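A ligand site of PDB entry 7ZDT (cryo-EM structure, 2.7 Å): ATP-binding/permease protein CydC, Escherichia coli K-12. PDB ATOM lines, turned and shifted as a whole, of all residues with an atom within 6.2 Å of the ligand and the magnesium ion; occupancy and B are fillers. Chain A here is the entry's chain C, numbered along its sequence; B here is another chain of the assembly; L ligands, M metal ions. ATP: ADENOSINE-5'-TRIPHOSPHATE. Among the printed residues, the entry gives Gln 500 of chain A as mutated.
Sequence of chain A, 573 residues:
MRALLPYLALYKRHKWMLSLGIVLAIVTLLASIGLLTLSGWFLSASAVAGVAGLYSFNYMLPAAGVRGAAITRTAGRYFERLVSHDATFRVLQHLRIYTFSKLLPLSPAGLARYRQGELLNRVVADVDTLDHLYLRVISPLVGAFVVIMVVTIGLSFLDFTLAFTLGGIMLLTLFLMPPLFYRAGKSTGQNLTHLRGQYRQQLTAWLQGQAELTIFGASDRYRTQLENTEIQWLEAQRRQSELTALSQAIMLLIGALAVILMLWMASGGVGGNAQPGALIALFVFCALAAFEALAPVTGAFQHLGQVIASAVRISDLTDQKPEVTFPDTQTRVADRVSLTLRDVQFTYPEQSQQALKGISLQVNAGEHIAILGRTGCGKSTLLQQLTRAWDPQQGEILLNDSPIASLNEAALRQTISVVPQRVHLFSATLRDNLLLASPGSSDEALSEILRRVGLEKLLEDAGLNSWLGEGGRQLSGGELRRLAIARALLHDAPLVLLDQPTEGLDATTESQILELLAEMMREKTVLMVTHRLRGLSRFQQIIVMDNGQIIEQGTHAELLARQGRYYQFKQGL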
ATOM      1  N   TYR A 348      -7.523 -10.726  26.284  1.00  0.00           N
ATOM      2  CA  TYR A 348      -8.661 -10.012  26.925  1.00  0.00           C
ATOM      3  C   TYR A 348      -9.701 -11.004  27.459  1.00  0.00           C
ATOM      4  O   TYR A 348      -9.787 -12.136  26.958  1.00  0.00           O
ATOM      5  CB  TYR A 348      -9.304  -9.016  25.967  1.00  0.00           C
ATOM      6  CG  TYR A 348      -8.665  -7.648  25.976  1.00  0.00           C
ATOM      7  CD1 TYR A 348      -8.954  -6.736  26.965  1.00  0.00           C
ATOM      8  CD2 TYR A 348      -7.773  -7.285  24.982  1.00  0.00           C
ATOM      9  CE1 TYR A 348      -8.372  -5.486  26.976  1.00  0.00           C
ATOM     10  CE2 TYR A 348      -7.186  -6.034  24.976  1.00  0.00           C
ATOM     11  CZ  TYR A 348      -7.484  -5.136  25.980  1.00  0.00           C
ATOM     12  OH  TYR A 348      -6.888  -3.907  25.956  1.00  0.00           O
ATOM     13  N   PRO A 349     -10.505 -10.617  28.464  1.00  0.00           N
ATOM     14  CA  PRO A 349     -11.532 -11.509  29.006  1.00  0.00           C
ATOM     15  C   PRO A 349     -12.545 -11.893  27.926  1.00  0.00           C
ATOM     16  O   PRO A 349     -12.902 -11.046  27.128  1.00  0.00           O
ATOM     17  CB  PRO A 349     -12.223 -10.633  30.056  1.00  0.00           C
ATOM     18  CG  PRO A 349     -11.183  -9.607  30.440  1.00  0.00           C
ATOM     19  CD  PRO A 349     -10.441  -9.334  29.155  1.00  0.00           C
ATOM     20  N   GLN A 351     -12.119 -13.800  25.326  1.00  0.00           N
ATOM     21  CA  GLN A 351     -11.512 -13.707  23.968  1.00  0.00           C
ATOM     22  C   GLN A 351     -10.647 -14.943  23.716  1.00  0.00           C
ATOM     23  O   GLN A 351     -10.290 -15.621  24.694  1.00  0.00           O
ATOM     24  CB  GLN A 351     -10.661 -12.448  23.824  1.00  0.00           C
ATOM     25  CG  GLN A 351     -11.351 -11.183  24.301  1.00  0.00           C
ATOM     26  CD  GLN A 351     -12.440 -10.756  23.362  1.00  0.00           C
ATOM     27  OE1 GLN A 351     -12.290 -10.795  22.142  1.00  0.00           O
ATOM     28  NE2 GLN A 351     -13.564 -10.347  23.928  1.00  0.00           N
ATOM     29  N   ALA A 355      -3.979 -10.179  22.478  1.00  0.00           N
ATOM     30  CA  ALA A 355      -3.727  -8.793  22.100  1.00  0.00           C
ATOM     31  C   ALA A 355      -2.236  -8.478  22.101  1.00  0.00           C
ATOM     32  O   ALA A 355      -1.772  -7.680  21.287  1.00  0.00           O
ATOM     33  CB  ALA A 355      -4.473  -7.850  23.034  1.00  0.00           C
ATOM     34  N   GLY A 373       2.548   1.752  14.945  1.00  0.00           N
ATOM     35  CA  GLY A 373       1.856   0.542  14.566  1.00  0.00           C
ATOM     36  C   GLY A 373       0.531   0.877  13.932  1.00  0.00           C
ATOM     37  O   GLY A 373       0.123   2.036  13.837  1.00  0.00           O
ATOM     38  N   ARG A 374      -0.146  -0.175  13.482  1.00  0.00           N
ATOM     39  CA  ARG A 374      -1.453  -0.050  12.867  1.00  0.00           C
ATOM     40  C   ARG A 374      -2.509   0.158  13.942  1.00  0.00           C
ATOM     41  O   ARG A 374      -2.265  -0.018  15.133  1.00  0.00           O
ATOM     42  CB  ARG A 374      -1.778  -1.297  12.061  1.00  0.00           C
ATOM     43  CG  ARG A 374      -0.724  -1.654  11.031  1.00  0.00           C
ATOM     44  CD  ARG A 374      -1.118  -1.290   9.620  1.00  0.00           C
ATOM     45  NE  ARG A 374      -0.308  -2.038   8.657  1.00  0.00           N
ATOM     46  CZ  ARG A 374      -0.427  -1.921   7.344  1.00  0.00           C
ATOM     47  NH1 ARG A 374       0.354  -2.643   6.538  1.00  0.00           N
ATOM     48  NH2 ARG A 374      -1.309  -1.085   6.828  1.00  0.00           N
ATOM     49  N   THR A 375      -3.705   0.553  13.512  1.00  0.00           N
ATOM     50  CA  THR A 375      -4.822   0.656  14.438  1.00  0.00           C
ATOM     51  C   THR A 375      -5.237  -0.729  14.904  1.00  0.00           C
ATOM     52  O   THR A 375      -5.356  -1.656  14.108  1.00  0.00           O
ATOM     53  CB  THR A 375      -5.998   1.370  13.781  1.00  0.00           C
ATOM     54  OG1 THR A 375      -6.293   0.765  12.526  1.00  0.00           O
ATOM     55  CG2 THR A 375      -5.656   2.830  13.556  1.00  0.00           C
ATOM     56  N   GLY A 376      -5.465  -0.863  16.211  1.00  0.00           N
ATOM     57  CA  GLY A 376      -5.814  -2.136  16.779  1.00  0.00           C
ATOM     58  C   GLY A 376      -4.675  -3.127  16.873  1.00  0.00           C
ATOM     59  O   GLY A 376      -4.923  -4.338  16.904  1.00  0.00           O
ATOM     60  N   CYS A 377      -3.438  -2.650  16.923  1.00  0.00           N
ATOM     61  CA  CYS A 377      -2.273  -3.524  16.995  1.00  0.00           C
ATOM     62  C   CYS A 377      -1.758  -3.709  18.422  1.00  0.00           C
ATOM     63  O   CYS A 377      -0.721  -4.337  18.617  1.00  0.00           O
ATOM     64  CB  CYS A 377      -1.156  -2.992  16.110  1.00  0.00           C
ATOM     65  SG  CYS A 377      -0.120  -1.743  16.876  1.00  0.00           S
ATOM     66  N   GLY A 378      -2.469  -3.192  19.424  1.00  0.00           N
ATOM     67  CA  GLY A 378      -2.074  -3.369  20.794  1.00  0.00           C
ATOM     68  C   GLY A 378      -1.254  -2.261  21.403  1.00  0.00           C
ATOM     69  O   GLY A 378      -0.650  -2.457  22.462  1.00  0.00           O
ATOM     70  N   LYS A 379      -1.223  -1.092  20.762  1.00  0.00           N
ATOM     71  CA  LYS A 379      -0.435   0.049  21.329  1.00  0.00           C
ATOM     72  C   LYS A 379      -1.040   0.443  22.678  1.00  0.00           C
ATOM     73  O   LYS A 379      -0.280   0.575  23.651  1.00  0.00           O
ATOM     74  CB  LYS A 379      -0.387   1.203  20.336  1.00  0.00           C
ATOM     75  CG  LYS A 379       0.344   0.908  19.026  1.00  0.00           C
ATOM     76  CD  LYS A 379       0.554   2.131  18.175  1.00  0.00           C
ATOM     77  CE  LYS A 379      -0.736   2.833  17.811  1.00  0.00           C
ATOM     78  NZ  LYS A 379      -1.676   1.913  17.135  1.00  0.00           N
ATOM     79  N   SER A 380      -2.369   0.624  22.731  1.00  0.00           N
ATOM     80  CA  SER A 380      -3.041   1.022  23.995  1.00  0.00           C
ATOM     81  C   SER A 380      -3.023  -0.125  25.013  1.00  0.00           C
ATOM     82  O   SER A 380      -3.000   0.163  26.228  1.00  0.00           O
ATOM     83  CB  SER A 380      -4.440   1.530  23.762  1.00  0.00           C
ATOM     84  OG  SER A 380      -4.441   2.934  23.563  1.00  0.00           O
ATOM     85  N   THR A 381      -3.081  -1.373  24.532  1.00  0.00           N
ATOM     86  CA  THR A 381      -3.016  -2.552  25.439  1.00  0.00           C
ATOM     87  C   THR A 381      -1.659  -2.598  26.159  1.00  0.00           C
ATOM     88  O   THR A 381      -1.626  -3.056  27.306  1.00  0.00           O
ATOM     89  CB  THR A 381      -3.401  -3.858  24.730  1.00  0.00           C
ATOM     90  OG1 THR A 381      -4.832  -3.885  24.697  1.00  0.00           O
ATOM     91  CG2 THR A 381      -2.907  -5.089  25.448  1.00  0.00           C
ATOM     92  N   LEU A 382      -0.586  -2.222  25.463  1.00  0.00           N
ATOM     93  CA  LEU A 382       0.769  -2.210  26.068  1.00  0.00           C
ATOM     94  C   LEU A 382       0.844  -1.154  27.172  1.00  0.00           C
ATOM     95  O   LEU A 382       1.271  -1.494  28.276  1.00  0.00           O
ATOM     96  CB  LEU A 382       1.796  -1.933  24.964  1.00  0.00           C
ATOM     97  CG  LEU A 382       3.257  -2.061  25.392  1.00  0.00           C
ATOM     98  CD1 LEU A 382       3.537  -3.455  25.914  1.00  0.00           C
ATOM     99  CD2 LEU A 382       4.184  -1.729  24.230  1.00  0.00           C
ATOM    100  N   TRP A 390      -4.271  -4.779  33.961  1.00  0.00           N
ATOM    101  CA  TRP A 390      -4.437  -6.223  33.989  1.00  0.00           C
ATOM    102  C   TRP A 390      -3.106  -6.845  34.385  1.00  0.00           C
ATOM    103  O   TRP A 390      -2.048  -6.234  34.225  1.00  0.00           O
ATOM    104  CB  TRP A 390      -4.850  -6.776  32.635  1.00  0.00           C
ATOM    105  CG  TRP A 390      -6.063  -6.149  32.067  1.00  0.00           C
ATOM    106  CD1 TRP A 390      -7.355  -6.446  32.351  1.00  0.00           C
ATOM    107  CD2 TRP A 390      -6.104  -5.113  31.080  1.00  0.00           C
ATOM    108  NE1 TRP A 390      -8.202  -5.648  31.619  1.00  0.00           N
ATOM    109  CE2 TRP A 390      -7.457  -4.824  30.831  1.00  0.00           C
ATOM    110  CE3 TRP A 390      -5.117  -4.392  30.395  1.00  0.00           C
ATOM    111  CZ2 TRP A 390      -7.845  -3.850  29.917  1.00  0.00           C
ATOM    112  CZ3 TRP A 390      -5.514  -3.433  29.496  1.00  0.00           C
ATOM    113  CH2 TRP A 390      -6.862  -3.165  29.269  1.00  0.00           C
ATOM    114  N   GLN A 421      -5.654   7.867  25.538  1.00  0.00           N
ATOM    115  CA  GLN A 421      -6.100   8.183  24.186  1.00  0.00           C
ATOM    116  C   GLN A 421      -7.459   8.875  24.193  1.00  0.00           C
ATOM    117  O   GLN A 421      -7.713   9.742  23.365  1.00  0.00           O
ATOM    118  CB  GLN A 421      -6.150   6.909  23.338  1.00  0.00           C
ATOM    119  CG  GLN A 421      -6.217   7.183  21.856  1.00  0.00           C
ATOM    120  CD  GLN A 421      -5.903   5.981  21.024  1.00  0.00           C
ATOM    121  OE1 GLN A 421      -5.553   4.926  21.540  1.00  0.00           O
ATOM    122  NE2 GLN A 421      -6.014   6.124  19.715  1.00  0.00           N
ATOM    123  N   ASP A 499      -0.290   8.331  25.120  1.00  0.00           N
ATOM    124  CA  ASP A 499      -1.002   7.614  24.034  1.00  0.00           C
ATOM    125  C   ASP A 499      -1.522   8.649  23.036  1.00  0.00           C
ATOM    126  O   ASP A 499      -2.604   9.203  23.279  1.00  0.00           O
ATOM    127  CB  ASP A 499      -2.153   6.788  24.615  1.00  0.00           C
ATOM    128  CG  ASP A 499      -2.482   5.523  23.836  1.00  0.00           C
ATOM    129  OD1 ASP A 499      -2.161   5.477  22.631  1.00  0.00           O
ATOM    130  OD2 ASP A 499      -3.060   4.602  24.437  1.00  0.00           O
ATOM    131  N   GLN A 500      -0.776   8.886  21.941  1.00  0.00           N
ATOM    132  CA  GLN A 500      -1.194   9.854  20.904  1.00  0.00           C
ATOM    133  C   GLN A 500      -1.566  11.197  21.548  1.00  0.00           C
ATOM    134  O   GLN A 500      -2.689  11.656  21.313  1.00  0.00           O
ATOM    135  CB  GLN A 500      -2.321   9.267  20.055  1.00  0.00           C
ATOM    136  CG  GLN A 500      -1.864   8.085  19.210  1.00  0.00           C
ATOM    137  CD  GLN A 500      -2.961   7.095  18.965  1.00  0.00           C
ATOM    138  OE1 GLN A 500      -4.084   7.461  18.618  1.00  0.00           O
ATOM    139  NE2 GLN A 500      -2.648   5.820  19.106  1.00  0.00           N
ATOM    140  N   VAL A 529       3.190   6.954  22.296  1.00  0.00           N
ATOM    141  CA  VAL A 529       2.530   6.288  21.175  1.00  0.00           C
ATOM    142  C   VAL A 529       2.098   7.356  20.187  1.00  0.00           C
ATOM    143  O   VAL A 529       1.422   8.321  20.559  1.00  0.00           O
ATOM    144  CB  VAL A 529       1.326   5.458  21.657  1.00  0.00           C
ATOM    145  CG1 VAL A 529       0.471   5.051  20.492  1.00  0.00           C
ATOM    146  CG2 VAL A 529       1.802   4.246  22.426  1.00  0.00           C
ATOM    147  N   HIS A 531       0.728   8.166  15.987  1.00  0.00           N
ATOM    148  CA  HIS A 531       0.381   7.860  14.609  1.00  0.00           C
ATOM    149  C   HIS A 531       1.013   8.854  13.645  1.00  0.00           C
ATOM    150  O   HIS A 531       0.711   8.823  12.447  1.00  0.00           O
ATOM    151  CB  HIS A 531      -1.134   7.849  14.417  1.00  0.00           C
ATOM    152  CG  HIS A 531      -1.787   6.585  14.885  1.00  0.00           C
ATOM    153  ND1 HIS A 531      -1.322   5.336  14.522  1.00  0.00           N
ATOM    154  CD2 HIS A 531      -2.872   6.371  15.655  1.00  0.00           C
ATOM    155  CE1 HIS A 531      -2.089   4.411  15.072  1.00  0.00           C
ATOM    156  NE2 HIS A 531      -3.042   5.010  15.763  1.00  0.00           N
ATOM    157  N   PHE B 467     -10.486  -5.736  10.453  1.00  0.00           N
ATOM    158  CA  PHE B 467     -10.407  -6.175  11.837  1.00  0.00           C
ATOM    159  C   PHE B 467     -11.629  -6.990  12.268  1.00  0.00           C
ATOM    160  O   PHE B 467     -11.749  -7.333  13.438  1.00  0.00           O
ATOM    161  CB  PHE B 467     -10.184  -4.991  12.778  1.00  0.00           C
ATOM    162  CG  PHE B 467     -11.370  -4.068  12.922  1.00  0.00           C
ATOM    163  CD1 PHE B 467     -12.387  -4.343  13.837  1.00  0.00           C
ATOM    164  CD2 PHE B 467     -11.437  -2.893  12.200  1.00  0.00           C
ATOM    165  CE1 PHE B 467     -13.459  -3.489  13.975  1.00  0.00           C
ATOM    166  CE2 PHE B 467     -12.505  -2.034  12.346  1.00  0.00           C
ATOM    167  CZ  PHE B 467     -13.516  -2.328  13.231  1.00  0.00           C
ATOM    168  N   LEU B 470     -10.867 -10.537  13.825  1.00  0.00           N
ATOM    169  CA  LEU B 470     -10.379 -10.487  15.196  1.00  0.00           C
ATOM    170  C   LEU B 470     -11.528 -10.604  16.187  1.00  0.00           C
ATOM    171  O   LEU B 470     -11.401 -11.249  17.232  1.00  0.00           O
ATOM    172  CB  LEU B 470      -9.599  -9.192  15.422  1.00  0.00           C
ATOM    173  CG  LEU B 470      -8.347  -9.003  14.562  1.00  0.00           C
ATOM    174  CD1 LEU B 470      -7.704  -7.662  14.834  1.00  0.00           C
ATOM    175  CD2 LEU B 470      -7.365 -10.132  14.805  1.00  0.00           C
ATOM    176  N   LEU B 471     -12.663  -9.965  15.883  1.00  0.00           N
ATOM    177  CA  LEU B 471     -13.793  -9.990  16.793  1.00  0.00           C
ATOM    178  C   LEU B 471     -14.386 -11.400  16.865  1.00  0.00           C
ATOM    179  O   LEU B 471     -14.415 -12.104  15.852  1.00  0.00           O
ATOM    180  CB  LEU B 471     -14.857  -8.993  16.340  1.00  0.00           C
ATOM    181  CG  LEU B 471     -14.341  -7.609  15.962  1.00  0.00           C
ATOM    182  CD1 LEU B 471     -15.494  -6.730  15.515  1.00  0.00           C
ATOM    183  CD2 LEU B 471     -13.608  -6.967  17.136  1.00  0.00           C
ATOM    184  N   ALA B 484     -16.028  -0.088  24.425  1.00  0.00           N
ATOM    185  CA  ALA B 484     -14.833  -0.540  25.126  1.00  0.00           C
ATOM    186  C   ALA B 484     -14.215  -1.745  24.442  1.00  0.00           C
ATOM    187  O   ALA B 484     -13.019  -2.008  24.592  1.00  0.00           O
ATOM    188  CB  ALA B 484     -15.175  -0.861  26.575  1.00  0.00           C
ATOM    189  N   ARG B 485     -15.019  -2.496  23.689  1.00  0.00           N
ATOM    190  CA  ARG B 485     -14.515  -3.664  22.978  1.00  0.00           C
ATOM    191  C   ARG B 485     -13.577  -3.281  21.842  1.00  0.00           C
ATOM    192  O   ARG B 485     -12.668  -4.060  21.511  1.00  0.00           O
ATOM    193  CB  ARG B 485     -15.683  -4.492  22.448  1.00  0.00           C
ATOM    194  CG  ARG B 485     -15.303  -5.692  21.616  1.00  0.00           C
ATOM    195  CD  ARG B 485     -14.379  -6.607  22.382  1.00  0.00           C
ATOM    196  NE  ARG B 485     -13.864  -7.705  21.556  1.00  0.00           N
ATOM    197  CZ  ARG B 485     -12.891  -7.570  20.662  1.00  0.00           C
ATOM    198  NH1 ARG B 485     -12.322  -6.391  20.464  1.00  0.00           N
ATOM    199  NH2 ARG B 485     -12.486  -8.615  19.968  1.00  0.00           N
ATOM    200  N   LEU B 486     -13.761  -2.117  21.244  1.00  0.00           N
ATOM    201  CA  LEU B 486     -12.952  -1.675  20.116  1.00  0.00           C
ATOM    202  C   LEU B 486     -11.855  -0.731  20.572  1.00  0.00           C
ATOM    203  O   LEU B 486     -11.959  -0.075  21.610  1.00  0.00           O
ATOM    204  CB  LEU B 486     -13.828  -0.977  19.070  1.00  0.00           C
ATOM    205  CG  LEU B 486     -15.003  -1.753  18.471  1.00  0.00           C
ATOM    206  CD1 LEU B 486     -15.837  -0.829  17.599  1.00  0.00           C
ATOM    207  CD2 LEU B 486     -14.506  -2.948  17.678  1.00  0.00           C
ATOM    208  N   SER B 487     -10.790  -0.672  19.781  1.00  0.00           N
ATOM    209  CA  SER B 487      -9.802   0.363  19.953  1.00  0.00           C
ATOM    210  C   SER B 487     -10.351   1.687  19.428  1.00  0.00           C
ATOM    211  O   SER B 487     -11.391   1.741  18.776  1.00  0.00           O
ATOM    212  CB  SER B 487      -8.500  -0.004  19.236  1.00  0.00           C
ATOM    213  OG  SER B 487      -8.561   0.339  17.865  1.00  0.00           O
ATOM    214  N   VAL B 488      -9.644   2.777  19.745  1.00  0.00           N
ATOM    215  CA  VAL B 488     -10.128   4.102  19.352  1.00  0.00           C
ATOM    216  C   VAL B 488     -10.206   4.228  17.840  1.00  0.00           C
ATOM    217  O   VAL B 488     -11.181   4.738  17.296  1.00  0.00           O
ATOM    218  CB  VAL B 488      -9.249   5.199  19.976  1.00  0.00           C
ATOM    219  CG1 VAL B 488      -9.693   6.558  19.501  1.00  0.00           C
ATOM    220  CG2 VAL B 488      -9.316   5.123  21.483  1.00  0.00           C
ATOM    221  N   GLY B 489      -9.181   3.739  17.132  1.00  0.00           N
ATOM    222  CA  GLY B 489      -9.189   3.803  15.686  1.00  0.00           C
ATOM    223  C   GLY B 489     -10.154   2.834  15.029  1.00  0.00           C
ATOM    224  O   GLY B 489     -10.548   3.053  13.879  1.00  0.00           O
ATOM    225  N   GLN B 490     -10.525   1.760  15.731  1.00  0.00           N
ATOM    226  CA  GLN B 490     -11.543   0.850  15.209  1.00  0.00           C
ATOM    227  C   GLN B 490     -12.935   1.445  15.347  1.00  0.00           C
ATOM    228  O   GLN B 490     -13.759   1.321  14.430  1.00  0.00           O
ATOM    229  CB  GLN B 490     -11.455  -0.499  15.912  1.00  0.00           C
ATOM    230  CG  GLN B 490     -10.146  -1.220  15.690  1.00  0.00           C
ATOM    231  CD  GLN B 490     -10.106  -2.582  16.337  1.00  0.00           C
ATOM    232  OE1 GLN B 490     -10.753  -2.818  17.350  1.00  0.00           O
ATOM    233  NE2 GLN B 490      -9.346  -3.494  15.741  1.00  0.00           N
ATOM    234  N   ARG B 493     -13.511   4.022  12.580  1.00  0.00           N
ATOM    235  CA  ARG B 493     -13.922   3.535  11.275  1.00  0.00           C
ATOM    236  C   ARG B 493     -15.354   3.006  11.287  1.00  0.00           C
ATOM    237  O   ARG B 493     -16.028   3.039  10.252  1.00  0.00           O
ATOM    238  CB  ARG B 493     -12.954   2.444  10.796  1.00  0.00           C
ATOM    239  CG  ARG B 493     -11.527   2.916  10.693  1.00  0.00           C
ATOM    240  CD  ARG B 493     -10.682   1.948   9.904  1.00  0.00           C
ATOM    241  NE  ARG B 493     -10.456   0.705  10.619  1.00  0.00           N
ATOM    242  CZ  ARG B 493      -9.400   0.482  11.396  1.00  0.00           C
ATOM    243  NH1 ARG B 493      -8.484   1.422  11.550  1.00  0.00           N
ATOM    244  NH2 ARG B 493      -9.271  -0.678  12.021  1.00  0.00           N
ATOM    245  N   SER B 515      -7.122   9.385  14.901  1.00  0.00           N
ATOM    246  CA  SER B 515      -6.589   8.203  15.580  1.00  0.00           C
ATOM    247  C   SER B 515      -6.330   7.056  14.613  1.00  0.00           C
ATOM    248  O   SER B 515      -6.386   5.883  14.982  1.00  0.00           O
ATOM    249  CB  SER B 515      -7.523   7.745  16.709  1.00  0.00           C
ATOM    250  OG  SER B 515      -7.098   6.510  17.234  1.00  0.00           O
ATOM    251  N   LEU B 516      -6.030   7.397  13.370  1.00  0.00           N
ATOM    252  CA  LEU B 516      -5.693   6.408  12.350  1.00  0.00           C
ATOM    253  C   LEU B 516      -4.243   6.609  11.937  1.00  0.00           C
ATOM    254  O   LEU B 516      -3.772   7.747  11.792  1.00  0.00           O
ATOM    255  CB  LEU B 516      -6.605   6.515  11.126  1.00  0.00           C
ATOM    256  CG  LEU B 516      -8.082   6.165  11.336  1.00  0.00           C
ATOM    257  CD1 LEU B 516      -8.816   6.207  10.015  1.00  0.00           C
ATOM    258  CD2 LEU B 516      -8.231   4.814  11.974  1.00  0.00           C
ATOM    259  N   ASP B 517      -3.536   5.505  11.740  1.00  0.00           N
ATOM    260  CA  ASP B 517      -2.144   5.588  11.328  1.00  0.00           C
ATOM    261  C   ASP B 517      -2.038   6.101   9.901  1.00  0.00           C
ATOM    262  O   ASP B 517      -3.035   6.412   9.245  1.00  0.00           O
ATOM    263  CB  ASP B 517      -1.442   4.239  11.459  1.00  0.00           C
ATOM    264  CG  ASP B 517      -2.119   3.155  10.652  1.00  0.00           C
ATOM    265  OD1 ASP B 517      -3.266   3.375  10.241  1.00  0.00           O
ATOM    266  OD2 ASP B 517      -1.503   2.098  10.423  1.00  0.00           O
HETATM  267  PG  ATP L   1      -5.511   2.449  17.959  1.00  0.00           P
HETATM  268  O1G ATP L   1      -5.758   3.287  19.168  1.00  0.00           O
HETATM  269  O2G ATP L   1      -4.236   2.814  17.250  1.00  0.00           O
HETATM  270  O3G ATP L   1      -6.683   2.420  17.028  1.00  0.00           O
HETATM  271  PB  ATP L   1      -4.351   0.267  19.555  1.00  0.00           P
HETATM  272  O1B ATP L   1      -4.269   1.149  20.738  1.00  0.00           O
HETATM  273  O2B ATP L   1      -3.100  -0.167  18.883  1.00  0.00           O
HETATM  274  O3B ATP L   1      -5.316   0.951  18.489  1.00  0.00           O
HETATM  275  PA  ATP L   1      -5.571  -1.697  21.365  1.00  0.00           P
HETATM  276  O1A ATP L   1      -4.318  -2.110  22.049  1.00  0.00           O
HETATM  277  O2A ATP L   1      -6.514  -0.816  22.094  1.00  0.00           O
HETATM  278  O3A ATP L   1      -5.230  -1.009  19.959  1.00  0.00           O
HETATM  279  O5' ATP L   1      -6.348  -2.998  20.881  1.00  0.00           O
HETATM  280  C5' ATP L   1      -5.651  -4.095  20.254  1.00  0.00           C
HETATM  281  C4' ATP L   1      -6.649  -5.191  19.983  1.00  0.00           C
HETATM  282  O4' ATP L   1      -7.393  -5.399  21.202  1.00  0.00           O
HETATM  283  C3' ATP L   1      -7.696  -4.879  18.911  1.00  0.00           C
HETATM  284  O3' ATP L   1      -8.122  -6.093  18.297  1.00  0.00           O
HETATM  285  C2' ATP L   1      -8.854  -4.346  19.757  1.00  0.00           C
HETATM  286  O2' ATP L   1     -10.105  -4.395  19.104  1.00  0.00           O
HETATM  287  C1' ATP L   1      -8.770  -5.296  20.939  1.00  0.00           C
HETATM  288  N9  ATP L   1      -9.414  -4.788  22.132  1.00  0.00           N
HETATM  289  C8  ATP L   1      -9.380  -3.503  22.617  1.00  0.00           C
HETATM  290  N7  ATP L   1     -10.075  -3.360  23.717  1.00  0.00           N
HETATM  291  C5  ATP L   1     -10.610  -4.617  23.959  1.00  0.00           C
HETATM  292  C6  ATP L   1     -11.443  -5.114  24.979  1.00  0.00           C
HETATM  293  N6  ATP L   1     -11.908  -4.385  25.986  1.00  0.00           N
HETATM  294  N1  ATP L   1     -11.784  -6.423  24.914  1.00  0.00           N
HETATM  295  C2  ATP L   1     -11.310  -7.162  23.908  1.00  0.00           C
HETATM  296  N3  ATP L   1     -10.525  -6.802  22.897  1.00  0.00           N
HETATM  297  C4  ATP L   1     -10.206  -5.499  22.992  1.00  0.00           C
HETATM  298 MG    MG M   1      -5.228   3.003  21.485  1.00  0.00          MG
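The side-chain amide nitrogen of Gln 421 sits at hydrogen-bond distance from the side-chain hydroxyl of Ser 515 of chain B (2.7 Å). The backbone carbonyl oxygen (O) of Arg 374 is in hydrogen-bond range of the side-chain amino group (NZ) of Lys 379 (2.8 Å). OG of Ser 515 of chain B is in hydrogen-bond range of N of Gly 489 of chain B, at 3.5 Å. OH of Tyr 348 is in hydrogen-bond range of OG1 of Thr 381 (2.4 Å). A ring nitrogen (NE2) of His 531 lies within hydrogen-bond range of the side-chain amide nitrogen (NE2) of Gln 500, 3.5 Å away. The side-chain amide nitrogen (NE2) of Gln 351 sits close to the backbone carbonyl oxygen (O) of Pro 349 (3.3 Å). The side-chain amide oxygen (OE1) of Gln 500 sits at hydrogen-bond distance from the side-chain hydroxyl (OG) of Ser 515 of chain B (3.5 Å). N of Gln 500 sits at hydrogen-bond distance from O of Val 529, 2.7 Å away.
An oxygen (O1A) of the ligand lies within hydrogen-bond range of the backbone NH (N) of Ser 380 (3.4 Å). The side-chain amide oxygen (OE1) of Gln 490 of chain B sits at hydrogen-bond distance from an oxygen (O2') of the ligand. An oxygen (O2B) of the ligand is in hydrogen-bond range of the backbone NH (N) of Lys 379 (2.8 Å). NZ of Lys 379 is in salt-bridge range of O2G of the ligand (2.7 Å). N of Gly 489 of chain B is in hydrogen-bond range of O3G of the ligand (2.8 Å). N of Gly 378 lies within hydrogen-bond range of O2B of the ligand (3.1 Å). An oxygen (O1A) of the ligand sits at hydrogen-bond distance from the backbone NH (N) of Thr 381, at 2.9 Å. O1A of the ligand is in hydrogen-bond range of OG1 of Thr 381, at 3.2 Å. O2G of the ligand sits at hydrogen-bond distance from NE2 of His 531 (2.9 Å). An oxygen (O3B) of the ligand sits at hydrogen-bond distance from the backbone NH (N) of Gly 376, 2.9 Å away. The side-chain hydroxyl (OG) of Ser 487 of chain B is in hydrogen-bond range of an oxygen (O3G) of the ligand. O of Ala 484 of chain B lies within hydrogen-bond range of N6 of the ligand. NH1 of Arg 485 of chain B lies within hydrogen-bond range of N3 of the ligand. An oxygen (O2B) of the ligand lies within hydrogen-bond range of the backbone NH (N) of Cys 377 (3.2 Å).
Asp 499 touches the magnesium ion. Three residues have an atom within 4 Å of the magnesium ion: Ser 380, Gln 421 and Asp 499.
CG of Tyr 348 touches C2 of the ligand, 3.4 Å away. Gln 351 touches the ligand (CD to C2, 3.8 Å). Arg 374 touches the ligand (O to O2B, 3.8 Å). Thr 375 touches the ligand (CB to O3G, 3.5 Å). Gln 500 touches the ligand. Leu 470 of chain B touches the ligand. Val 488 of chain B touches the ligand. Ser 515 of chain B touches the ligand (OG to O1G, 3.99 Å). Hydrophobic or aromatic side chains within 4 Å of the ligand: Tyr 348, His 531 and Leu 470 of chain B. Within 4 Å of the ligand: Tyr 348, Gln 351, Arg 374, Thr 375, Gly 376, Cys 377, Gly 378, Lys 379, Ser 380, Thr 381, Gln 421, Gln 500, His 531, Leu 470 of chain B, Ala 484 of chain B, Arg 485 of chain B, Ser 487 of chain B, Val 488 of chain B, Gly 489 of chain B, Gln 490 of chain B and Ser 515 of chain B.
The magnesium ion is bound by the side-chain amide oxygen of Gln 421 (2.0 Å), an oxygen (O1B) of the ligand (2.2 Å), the side-chain hydroxyl of Ser 380 (2.2 Å) and an oxygen (O1G) of the ligand (2.4 Å). The magnesium ion has four donor atoms within binding distance.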
